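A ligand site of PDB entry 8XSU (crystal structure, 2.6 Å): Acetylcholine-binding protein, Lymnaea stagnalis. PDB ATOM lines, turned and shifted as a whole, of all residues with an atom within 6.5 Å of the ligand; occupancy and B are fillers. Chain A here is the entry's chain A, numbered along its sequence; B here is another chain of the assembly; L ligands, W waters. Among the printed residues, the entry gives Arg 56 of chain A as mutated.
The side-chain sulfur (SG) of Cys 188 of chain B lies close to an oxygen (O2) of the ligand, at 2.6 Å.
Trp 54 touches the ligand.
Arg 56 touches the ligand.
NE1 of Trp 144 of chain B touches C4 of the ligand (3.3 Å).
Thr 145 of chain B touches the ligand (CG2 to O3, 3.7 Å).
CZ of Tyr 186 of chain B touches C6 of the ligand (3.2 Å).
OH of Tyr 193 of chain B touches C2 of the ligand, 3.7 Å away.
Within 4 Å of the ligand: Lys 35, Trp 54, Arg 56, Met 115, Trp 144 of chain B, Thr 145 of chain B, Tyr 186 of chain B, Cys 188 of chain B and Tyr 193 of chain B.
Water W1 lies within hydrogen-bond range of O of Leu 103 (2.9 Å), O3 of the ligand (3.0 Å), N of Met 115 (3.0 Å) and NE1 of Trp 144 of chain B (3.4 Å).
The side-chain sulfur (SG) of Cys 189 of chain B is disulfide-bonded to the side-chain sulfur (SG) of Cys 188 of chain B, at 2.1 Å.
O of Met 115 sits at hydrogen-bond distance from NE1 of Trp 144 of chain B, at 2.9 Å.
The backbone carbonyl oxygen (O) of Lys 35 sits at hydrogen-bond distance from the backbone NH (N) of Trp 54 (2.8 Å).
NZ of Lys 35 lies within salt-bridge range of OE1 of Glu 158 (3.6 Å).
The guanidinium group of Arg 105 sits at hydrogen-bond distance from the backbone carbonyl oxygen of Thr 145 of chain B (3.4 Å).
N of Thr 145 of chain B lies within hydrogen-bond range of OG of Ser 143 of chain B, at 3.4 Å.
SD of Met 115 sits close to N1 of the ligand, at 3.8 Å.
O1 of the ligand sits at hydrogen-bond distance from NZ of Lys 35, 3.3 Å away.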
ATOM      1  N   LYS A  35      -7.642  15.911  31.122  1.00  0.00           N
ATOM      2  CA  LYS A  35      -8.074  17.228  31.556  1.00  0.00           C
ATOM      3  C   LYS A  35      -9.100  17.771  30.551  1.00  0.00           C
ATOM      4  O   LYS A  35      -8.791  17.942  29.374  1.00  0.00           O
ATOM      5  CB  LYS A  35      -6.915  18.212  31.693  1.00  0.00           C
ATOM      6  CG  LYS A  35      -6.147  18.181  32.998  1.00  0.00           C
ATOM      7  CD  LYS A  35      -5.178  16.992  33.015  1.00  0.00           C
ATOM      8  CE  LYS A  35      -3.928  17.162  32.167  1.00  0.00           C
ATOM      9  NZ  LYS A  35      -2.999  18.129  32.761  1.00  0.00           N
ATOM     10  N   TRP A  54      -7.467  17.163  27.006  1.00  0.00           N
ATOM     11  CA  TRP A  54      -6.065  16.831  26.919  1.00  0.00           C
ATOM     12  C   TRP A  54      -5.834  15.457  27.525  1.00  0.00           C
ATOM     13  O   TRP A  54      -6.153  15.261  28.685  1.00  0.00           O
ATOM     14  CB  TRP A  54      -5.228  17.861  27.686  1.00  0.00           C
ATOM     15  CG  TRP A  54      -5.380  19.268  27.205  1.00  0.00           C
ATOM     16  CD1 TRP A  54      -5.866  19.679  26.000  1.00  0.00           C
ATOM     17  CD2 TRP A  54      -4.993  20.458  27.905  1.00  0.00           C
ATOM     18  NE1 TRP A  54      -5.809  21.038  25.899  1.00  0.00           N
ATOM     19  CE2 TRP A  54      -5.276  21.549  27.055  1.00  0.00           C
ATOM     20  CE3 TRP A  54      -4.437  20.711  29.165  1.00  0.00           C
ATOM     21  CZ2 TRP A  54      -5.025  22.869  27.414  1.00  0.00           C
ATOM     22  CZ3 TRP A  54      -4.161  22.011  29.513  1.00  0.00           C
ATOM     23  CH2 TRP A  54      -4.455  23.078  28.647  1.00  0.00           C
ATOM     24  N   ARG A  56      -3.277  13.323  28.823  1.00  0.00           N
ATOM     25  CA  ARG A  56      -1.911  13.232  29.297  1.00  0.00           C
ATOM     26  C   ARG A  56      -1.508  11.765  29.367  1.00  0.00           C
ATOM     27  O   ARG A  56      -2.098  10.999  30.122  1.00  0.00           O
ATOM     28  CB  ARG A  56      -1.829  13.949  30.648  1.00  0.00           C
ATOM     29  CG  ARG A  56      -0.392  14.155  31.118  1.00  0.00           C
ATOM     30  CD  ARG A  56      -0.306  15.157  32.266  1.00  0.00           C
ATOM     31  NE  ARG A  56       1.091  15.495  32.562  1.00  0.00           N
ATOM     32  CZ  ARG A  56       2.015  14.642  33.018  1.00  0.00           C
ATOM     33  NH1 ARG A  56       1.672  13.416  33.411  1.00  0.00           N
ATOM     34  NH2 ARG A  56       3.278  15.044  33.155  1.00  0.00           N
ATOM     35  N   LEU A 103       3.556  15.720  18.512  1.00  0.00           N
ATOM     36  CA  LEU A 103       4.894  15.634  19.062  1.00  0.00           C
ATOM     37  C   LEU A 103       4.799  15.155  20.504  1.00  0.00           C
ATOM     38  O   LEU A 103       3.917  15.581  21.249  1.00  0.00           O
ATOM     39  CB  LEU A 103       5.513  17.021  18.992  1.00  0.00           C
ATOM     40  CG  LEU A 103       5.684  17.637  17.599  1.00  0.00           C
ATOM     41  CD1 LEU A 103       6.434  18.938  17.625  1.00  0.00           C
ATOM     42  CD2 LEU A 103       6.429  16.668  16.713  1.00  0.00           C
ATOM     43  N   ALA A 104       5.700  14.277  20.909  1.00  0.00           N
ATOM     44  CA  ALA A 104       5.832  13.915  22.314  1.00  0.00           C
ATOM     45  C   ALA A 104       7.121  14.506  22.873  1.00  0.00           C
ATOM     46  O   ALA A 104       7.993  14.930  22.148  1.00  0.00           O
ATOM     47  CB  ALA A 104       5.837  12.403  22.475  1.00  0.00           C
ATOM     48  N   ARG A 105       7.250  14.484  24.183  1.00  0.00           N
ATOM     49  CA  ARG A 105       8.433  15.016  24.851  1.00  0.00           C
ATOM     50  C   ARG A 105       9.180  13.833  25.440  1.00  0.00           C
ATOM     51  O   ARG A 105       8.577  12.988  26.073  1.00  0.00           O
ATOM     52  CB  ARG A 105       7.873  15.992  25.872  1.00  0.00           C
ATOM     53  CG  ARG A 105       8.848  17.060  26.315  1.00  0.00           C
ATOM     54  CD  ARG A 105       8.992  18.233  25.373  1.00  0.00           C
ATOM     55  NE  ARG A 105      10.029  19.054  26.000  1.00  0.00           N
ATOM     56  CZ  ARG A 105      10.901  19.796  25.369  1.00  0.00           C
ATOM     57  NH1 ARG A 105      10.811  19.939  24.070  1.00  0.00           N
ATOM     58  NH2 ARG A 105      11.863  20.397  26.038  1.00  0.00           N
ATOM     59  N   LEU A 113       6.339  11.842  27.410  1.00  0.00           N
ATOM     60  CA  LEU A 113       5.078  12.498  27.693  1.00  0.00           C
ATOM     61  C   LEU A 113       4.412  12.885  26.378  1.00  0.00           C
ATOM     62  O   LEU A 113       4.949  13.700  25.625  1.00  0.00           O
ATOM     63  CB  LEU A 113       5.375  13.737  28.547  1.00  0.00           C
ATOM     64  CG  LEU A 113       4.234  14.735  28.716  1.00  0.00           C
ATOM     65  CD1 LEU A 113       2.942  14.107  29.233  1.00  0.00           C
ATOM     66  CD2 LEU A 113       4.700  15.805  29.670  1.00  0.00           C
ATOM     67  N   TYR A 114       3.258  12.288  26.108  1.00  0.00           N
ATOM     68  CA  TYR A 114       2.452  12.625  24.951  1.00  0.00           C
ATOM     69  C   TYR A 114       1.123  13.155  25.470  1.00  0.00           C
ATOM     70  O   TYR A 114       0.462  12.496  26.272  1.00  0.00           O
ATOM     71  CB  TYR A 114       2.260  11.438  23.994  1.00  0.00           C
ATOM     72  CG  TYR A 114       1.470  11.769  22.727  1.00  0.00           C
ATOM     73  CD1 TYR A 114       1.713  12.923  22.006  1.00  0.00           C
ATOM     74  CD2 TYR A 114       0.451  10.934  22.264  1.00  0.00           C
ATOM     75  CE1 TYR A 114       0.978  13.248  20.879  1.00  0.00           C
ATOM     76  CE2 TYR A 114      -0.275  11.248  21.140  1.00  0.00           C
ATOM     77  CZ  TYR A 114      -0.015  12.404  20.437  1.00  0.00           C
ATOM     78  OH  TYR A 114      -0.701  12.741  19.290  1.00  0.00           O
ATOM     79  N   MET A 115       0.767  14.372  25.044  1.00  0.00           N
ATOM     80  CA  MET A 115      -0.423  15.015  25.558  1.00  0.00           C
ATOM     81  C   MET A 115      -1.152  15.761  24.445  1.00  0.00           C
ATOM     82  O   MET A 115      -1.143  16.992  24.409  1.00  0.00           O
ATOM     83  CB  MET A 115      -0.099  15.966  26.711  1.00  0.00           C
ATOM     84  CG  MET A 115      -1.344  16.478  27.404  1.00  0.00           C
ATOM     85  SD  MET A 115      -0.852  17.485  28.810  1.00  0.00           S
ATOM     86  CE  MET A 115      -2.196  18.658  28.702  1.00  0.00           C
ATOM     87  N   PRO A 116      -1.823  15.037  23.529  1.00  0.00           N
ATOM     88  CA  PRO A 116      -2.650  15.643  22.501  1.00  0.00           C
ATOM     89  C   PRO A 116      -3.951  16.191  23.060  1.00  0.00           C
ATOM     90  O   PRO A 116      -4.500  15.608  23.993  1.00  0.00           O
ATOM     91  CB  PRO A 116      -2.880  14.461  21.586  1.00  0.00           C
ATOM     92  CG  PRO A 116      -3.035  13.318  22.537  1.00  0.00           C
ATOM     93  CD  PRO A 116      -1.905  13.580  23.515  1.00  0.00           C
ATOM     94  N   GLU A 158      -3.168  13.528  39.783  1.00  0.00           N
ATOM     95  CA  GLU A 158      -3.255  14.969  39.648  1.00  0.00           C
ATOM     96  C   GLU A 158      -4.074  15.533  40.796  1.00  0.00           C
ATOM     97  O   GLU A 158      -3.685  16.541  41.351  1.00  0.00           O
ATOM     98  CB  GLU A 158      -3.928  15.294  38.316  1.00  0.00           C
ATOM     99  CG  GLU A 158      -3.101  14.860  37.107  1.00  0.00           C
ATOM    100  CD  GLU A 158      -3.696  15.190  35.747  1.00  0.00           C
ATOM    101  OE1 GLU A 158      -2.913  15.106  34.777  1.00  0.00           O
ATOM    102  OE2 GLU A 158      -4.913  15.499  35.627  1.00  0.00           O
ATOM    103  N   TYR A 165      -8.702  23.907  33.507  1.00  0.00           N
ATOM    104  CA  TYR A 165      -8.381  24.307  32.152  1.00  0.00           C
ATOM    105  C   TYR A 165      -9.644  24.314  31.289  1.00  0.00           C
ATOM    106  O   TYR A 165      -9.580  24.498  30.073  1.00  0.00           O
ATOM    107  CB  TYR A 165      -7.292  23.329  31.710  1.00  0.00           C
ATOM    108  CG  TYR A 165      -6.032  23.360  32.572  1.00  0.00           C
ATOM    109  CD1 TYR A 165      -5.434  24.567  32.917  1.00  0.00           C
ATOM    110  CD2 TYR A 165      -5.469  22.186  33.082  1.00  0.00           C
ATOM    111  CE1 TYR A 165      -4.308  24.614  33.723  1.00  0.00           C
ATOM    112  CE2 TYR A 165      -4.327  22.224  33.874  1.00  0.00           C
ATOM    113  CZ  TYR A 165      -3.752  23.446  34.205  1.00  0.00           C
ATOM    114  OH  TYR A 165      -2.645  23.529  34.994  1.00  0.00           O
ATOM    115  N   TYR B  90      -4.843  27.333  21.484  1.00  0.00           N
ATOM    116  CA  TYR B  90      -5.130  26.643  22.733  1.00  0.00           C
ATOM    117  C   TYR B  90      -6.640  26.484  22.934  1.00  0.00           C
ATOM    118  O   TYR B  90      -7.057  25.565  23.627  1.00  0.00           O
ATOM    119  CB  TYR B  90      -4.526  27.343  23.954  1.00  0.00           C
ATOM    120  CG  TYR B  90      -3.007  27.277  24.121  1.00  0.00           C
ATOM    121  CD1 TYR B  90      -2.143  27.355  23.030  1.00  0.00           C
ATOM    122  CD2 TYR B  90      -2.429  27.146  25.365  1.00  0.00           C
ATOM    123  CE1 TYR B  90      -0.768  27.297  23.179  1.00  0.00           C
ATOM    124  CE2 TYR B  90      -1.050  27.078  25.534  1.00  0.00           C
ATOM    125  CZ  TYR B  90      -0.218  27.164  24.439  1.00  0.00           C
ATOM    126  OH  TYR B  90       1.140  27.104  24.570  1.00  0.00           O
ATOM    127  N   SER B 143       3.493  27.606  21.183  1.00  0.00           N
ATOM    128  CA  SER B 143       4.046  26.277  20.996  1.00  0.00           C
ATOM    129  C   SER B 143       3.291  25.283  21.854  1.00  0.00           C
ATOM    130  O   SER B 143       2.935  25.583  22.979  1.00  0.00           O
ATOM    131  CB  SER B 143       5.527  26.227  21.303  1.00  0.00           C
ATOM    132  OG  SER B 143       6.021  24.888  21.340  1.00  0.00           O
ATOM    133  N   TRP B 144       3.089  24.067  21.313  1.00  0.00           N
ATOM    134  CA  TRP B 144       2.437  23.036  22.083  1.00  0.00           C
ATOM    135  C   TRP B 144       3.438  22.320  22.990  1.00  0.00           C
ATOM    136  O   TRP B 144       3.088  22.017  24.125  1.00  0.00           O
ATOM    137  CB  TRP B 144       1.673  22.063  21.171  1.00  0.00           C
ATOM    138  CG  TRP B 144       0.813  21.104  21.946  1.00  0.00           C
ATOM    139  CD1 TRP B 144       1.007  19.757  22.120  1.00  0.00           C
ATOM    140  CD2 TRP B 144      -0.342  21.438  22.731  1.00  0.00           C
ATOM    141  NE1 TRP B 144       0.035  19.232  22.930  1.00  0.00           N
ATOM    142  CE2 TRP B 144      -0.794  20.246  23.326  1.00  0.00           C
ATOM    143  CE3 TRP B 144      -1.022  22.623  22.981  1.00  0.00           C
ATOM    144  CZ2 TRP B 144      -1.911  20.213  24.169  1.00  0.00           C
ATOM    145  CZ3 TRP B 144      -2.113  22.597  23.833  1.00  0.00           C
ATOM    146  CH2 TRP B 144      -2.534  21.405  24.426  1.00  0.00           C
ATOM    147  N   THR B 145       4.666  22.058  22.517  1.00  0.00           N
ATOM    148  CA  THR B 145       5.624  21.224  23.266  1.00  0.00           C
ATOM    149  C   THR B 145       6.932  21.956  23.628  1.00  0.00           C
ATOM    150  O   THR B 145       7.716  21.376  24.375  1.00  0.00           O
ATOM    151  CB  THR B 145       5.950  19.950  22.475  1.00  0.00           C
ATOM    152  OG1 THR B 145       6.655  20.297  21.283  1.00  0.00           O
ATOM    153  CG2 THR B 145       4.708  19.164  22.121  1.00  0.00           C
ATOM    154  N   HIS B 146       7.181  23.185  23.143  1.00  0.00           N
ATOM    155  CA  HIS B 146       8.429  23.865  23.454  1.00  0.00           C
ATOM    156  C   HIS B 146       8.212  25.034  24.419  1.00  0.00           C
ATOM    157  O   HIS B 146       7.519  25.991  24.109  1.00  0.00           O
ATOM    158  CB  HIS B 146       9.116  24.393  22.188  1.00  0.00           C
ATOM    159  CG  HIS B 146       9.575  23.324  21.246  1.00  0.00           C
ATOM    160  ND1 HIS B 146      10.722  22.617  21.471  1.00  0.00           N
ATOM    161  CD2 HIS B 146       9.056  22.850  20.108  1.00  0.00           C
ATOM    162  CE1 HIS B 146      10.894  21.756  20.469  1.00  0.00           C
ATOM    163  NE2 HIS B 146       9.894  21.893  19.637  1.00  0.00           N
ATOM    164  N   TYR B 186       1.835  25.178  33.839  1.00  0.00           N
ATOM    165  CA  TYR B 186       0.961  24.106  34.277  1.00  0.00           C
ATOM    166  C   TYR B 186       1.466  23.607  35.633  1.00  0.00           C
ATOM    167  O   TYR B 186       2.668  23.568  35.865  1.00  0.00           O
ATOM    168  CB  TYR B 186       0.845  23.048  33.173  1.00  0.00           C
ATOM    169  CG  TYR B 186       0.295  23.618  31.865  1.00  0.00           C
ATOM    170  CD1 TYR B 186      -1.060  23.825  31.647  1.00  0.00           C
ATOM    171  CD2 TYR B 186       1.166  23.951  30.833  1.00  0.00           C
ATOM    172  CE1 TYR B 186      -1.541  24.379  30.466  1.00  0.00           C
ATOM    173  CE2 TYR B 186       0.698  24.482  29.636  1.00  0.00           C
ATOM    174  CZ  TYR B 186      -0.652  24.714  29.451  1.00  0.00           C
ATOM    175  OH  TYR B 186      -1.050  25.247  28.273  1.00  0.00           O
ATOM    176  N   SER B 187       0.520  23.258  36.512  1.00  0.00           N
ATOM    177  CA  SER B 187       0.828  22.907  37.891  1.00  0.00           C
ATOM    178  C   SER B 187       1.704  21.654  37.961  1.00  0.00           C
ATOM    179  O   SER B 187       2.402  21.464  38.951  1.00  0.00           O
ATOM    180  CB  SER B 187      -0.435  22.718  38.680  1.00  0.00           C
ATOM    181  OG  SER B 187      -1.262  21.769  38.022  1.00  0.00           O
ATOM    182  N   CYS B 188       1.666  20.811  36.925  1.00  0.00           N
ATOM    183  CA  CYS B 188       2.519  19.632  36.843  1.00  0.00           C
ATOM    184  C   CYS B 188       4.004  19.993  36.999  1.00  0.00           C
ATOM    185  O   CYS B 188       4.755  19.225  37.595  1.00  0.00           O
ATOM    186  CB  CYS B 188       2.334  18.893  35.517  1.00  0.00           C
ATOM    187  SG  CYS B 188       3.099  19.699  34.085  1.00  0.00           S
ATOM    188  N   CYS B 189       4.411  21.154  36.449  1.00  0.00           N
ATOM    189  CA  CYS B 189       5.778  21.373  36.031  1.00  0.00           C
ATOM    190  C   CYS B 189       6.152  22.847  36.173  1.00  0.00           C
ATOM    191  O   CYS B 189       5.275  23.719  36.244  1.00  0.00           O
ATOM    192  CB  CYS B 189       5.944  20.897  34.593  1.00  0.00           C
ATOM    193  SG  CYS B 189       5.128  19.319  34.244  1.00  0.00           S
ATOM    194  N   TYR B 193       4.994  28.213  28.862  1.00  0.00           N
ATOM    195  CA  TYR B 193       4.760  28.186  27.424  1.00  0.00           C
ATOM    196  C   TYR B 193       4.279  29.564  27.003  1.00  0.00           C
ATOM    197  O   TYR B 193       3.243  30.032  27.442  1.00  0.00           O
ATOM    198  CB  TYR B 193       3.789  27.048  27.072  1.00  0.00           C
ATOM    199  CG  TYR B 193       4.346  25.674  27.428  1.00  0.00           C
ATOM    200  CD1 TYR B 193       4.288  25.179  28.729  1.00  0.00           C
ATOM    201  CD2 TYR B 193       4.993  24.911  26.472  1.00  0.00           C
ATOM    202  CE1 TYR B 193       4.823  23.944  29.056  1.00  0.00           C
ATOM    203  CE2 TYR B 193       5.550  23.686  26.795  1.00  0.00           C
ATOM    204  CZ  TYR B 193       5.444  23.191  28.080  1.00  0.00           C
ATOM    205  OH  TYR B 193       6.005  21.982  28.375  1.00  0.00           O
HETATM  206  C1  LIG L   1       2.511  19.447  26.746  1.00  0.00           C
HETATM  207  C2  LIG L   1       4.031  19.234  26.916  1.00  0.00           C
HETATM  208  C3  LIG L   1       4.271  18.008  26.090  1.00  0.00           C
HETATM  209  C4  LIG L   1       2.334  18.991  25.297  1.00  0.00           C
HETATM  210  N1  LIG L   1      -0.281  21.175  29.263  1.00  0.00           N
HETATM  211  N2  LIG L   1       1.408  20.198  30.613  1.00  0.00           N
HETATM  212  C5  LIG L   1       1.987  20.821  27.127  1.00  0.00           C
HETATM  213  N3  LIG L   1       0.563  19.857  31.599  1.00  0.00           N
HETATM  214  C6  LIG L   1      -0.780  21.843  28.085  1.00  0.00           C
HETATM  215  C7  LIG L   1       0.993  20.806  29.468  1.00  0.00           C
HETATM  216  O1  LIG L   1      -0.647  20.110  31.505  1.00  0.00           O
HETATM  217  O2  LIG L   1       1.034  19.273  32.606  1.00  0.00           O
HETATM  218  N4  LIG L   1       1.999  20.739  28.579  1.00  0.00           N
HETATM  219  O3  LIG L   1       3.165  17.837  25.166  1.00  0.00           O
HETATM  220  O   HOH W   1       1.770  16.339  22.968  1.00  0.00           O
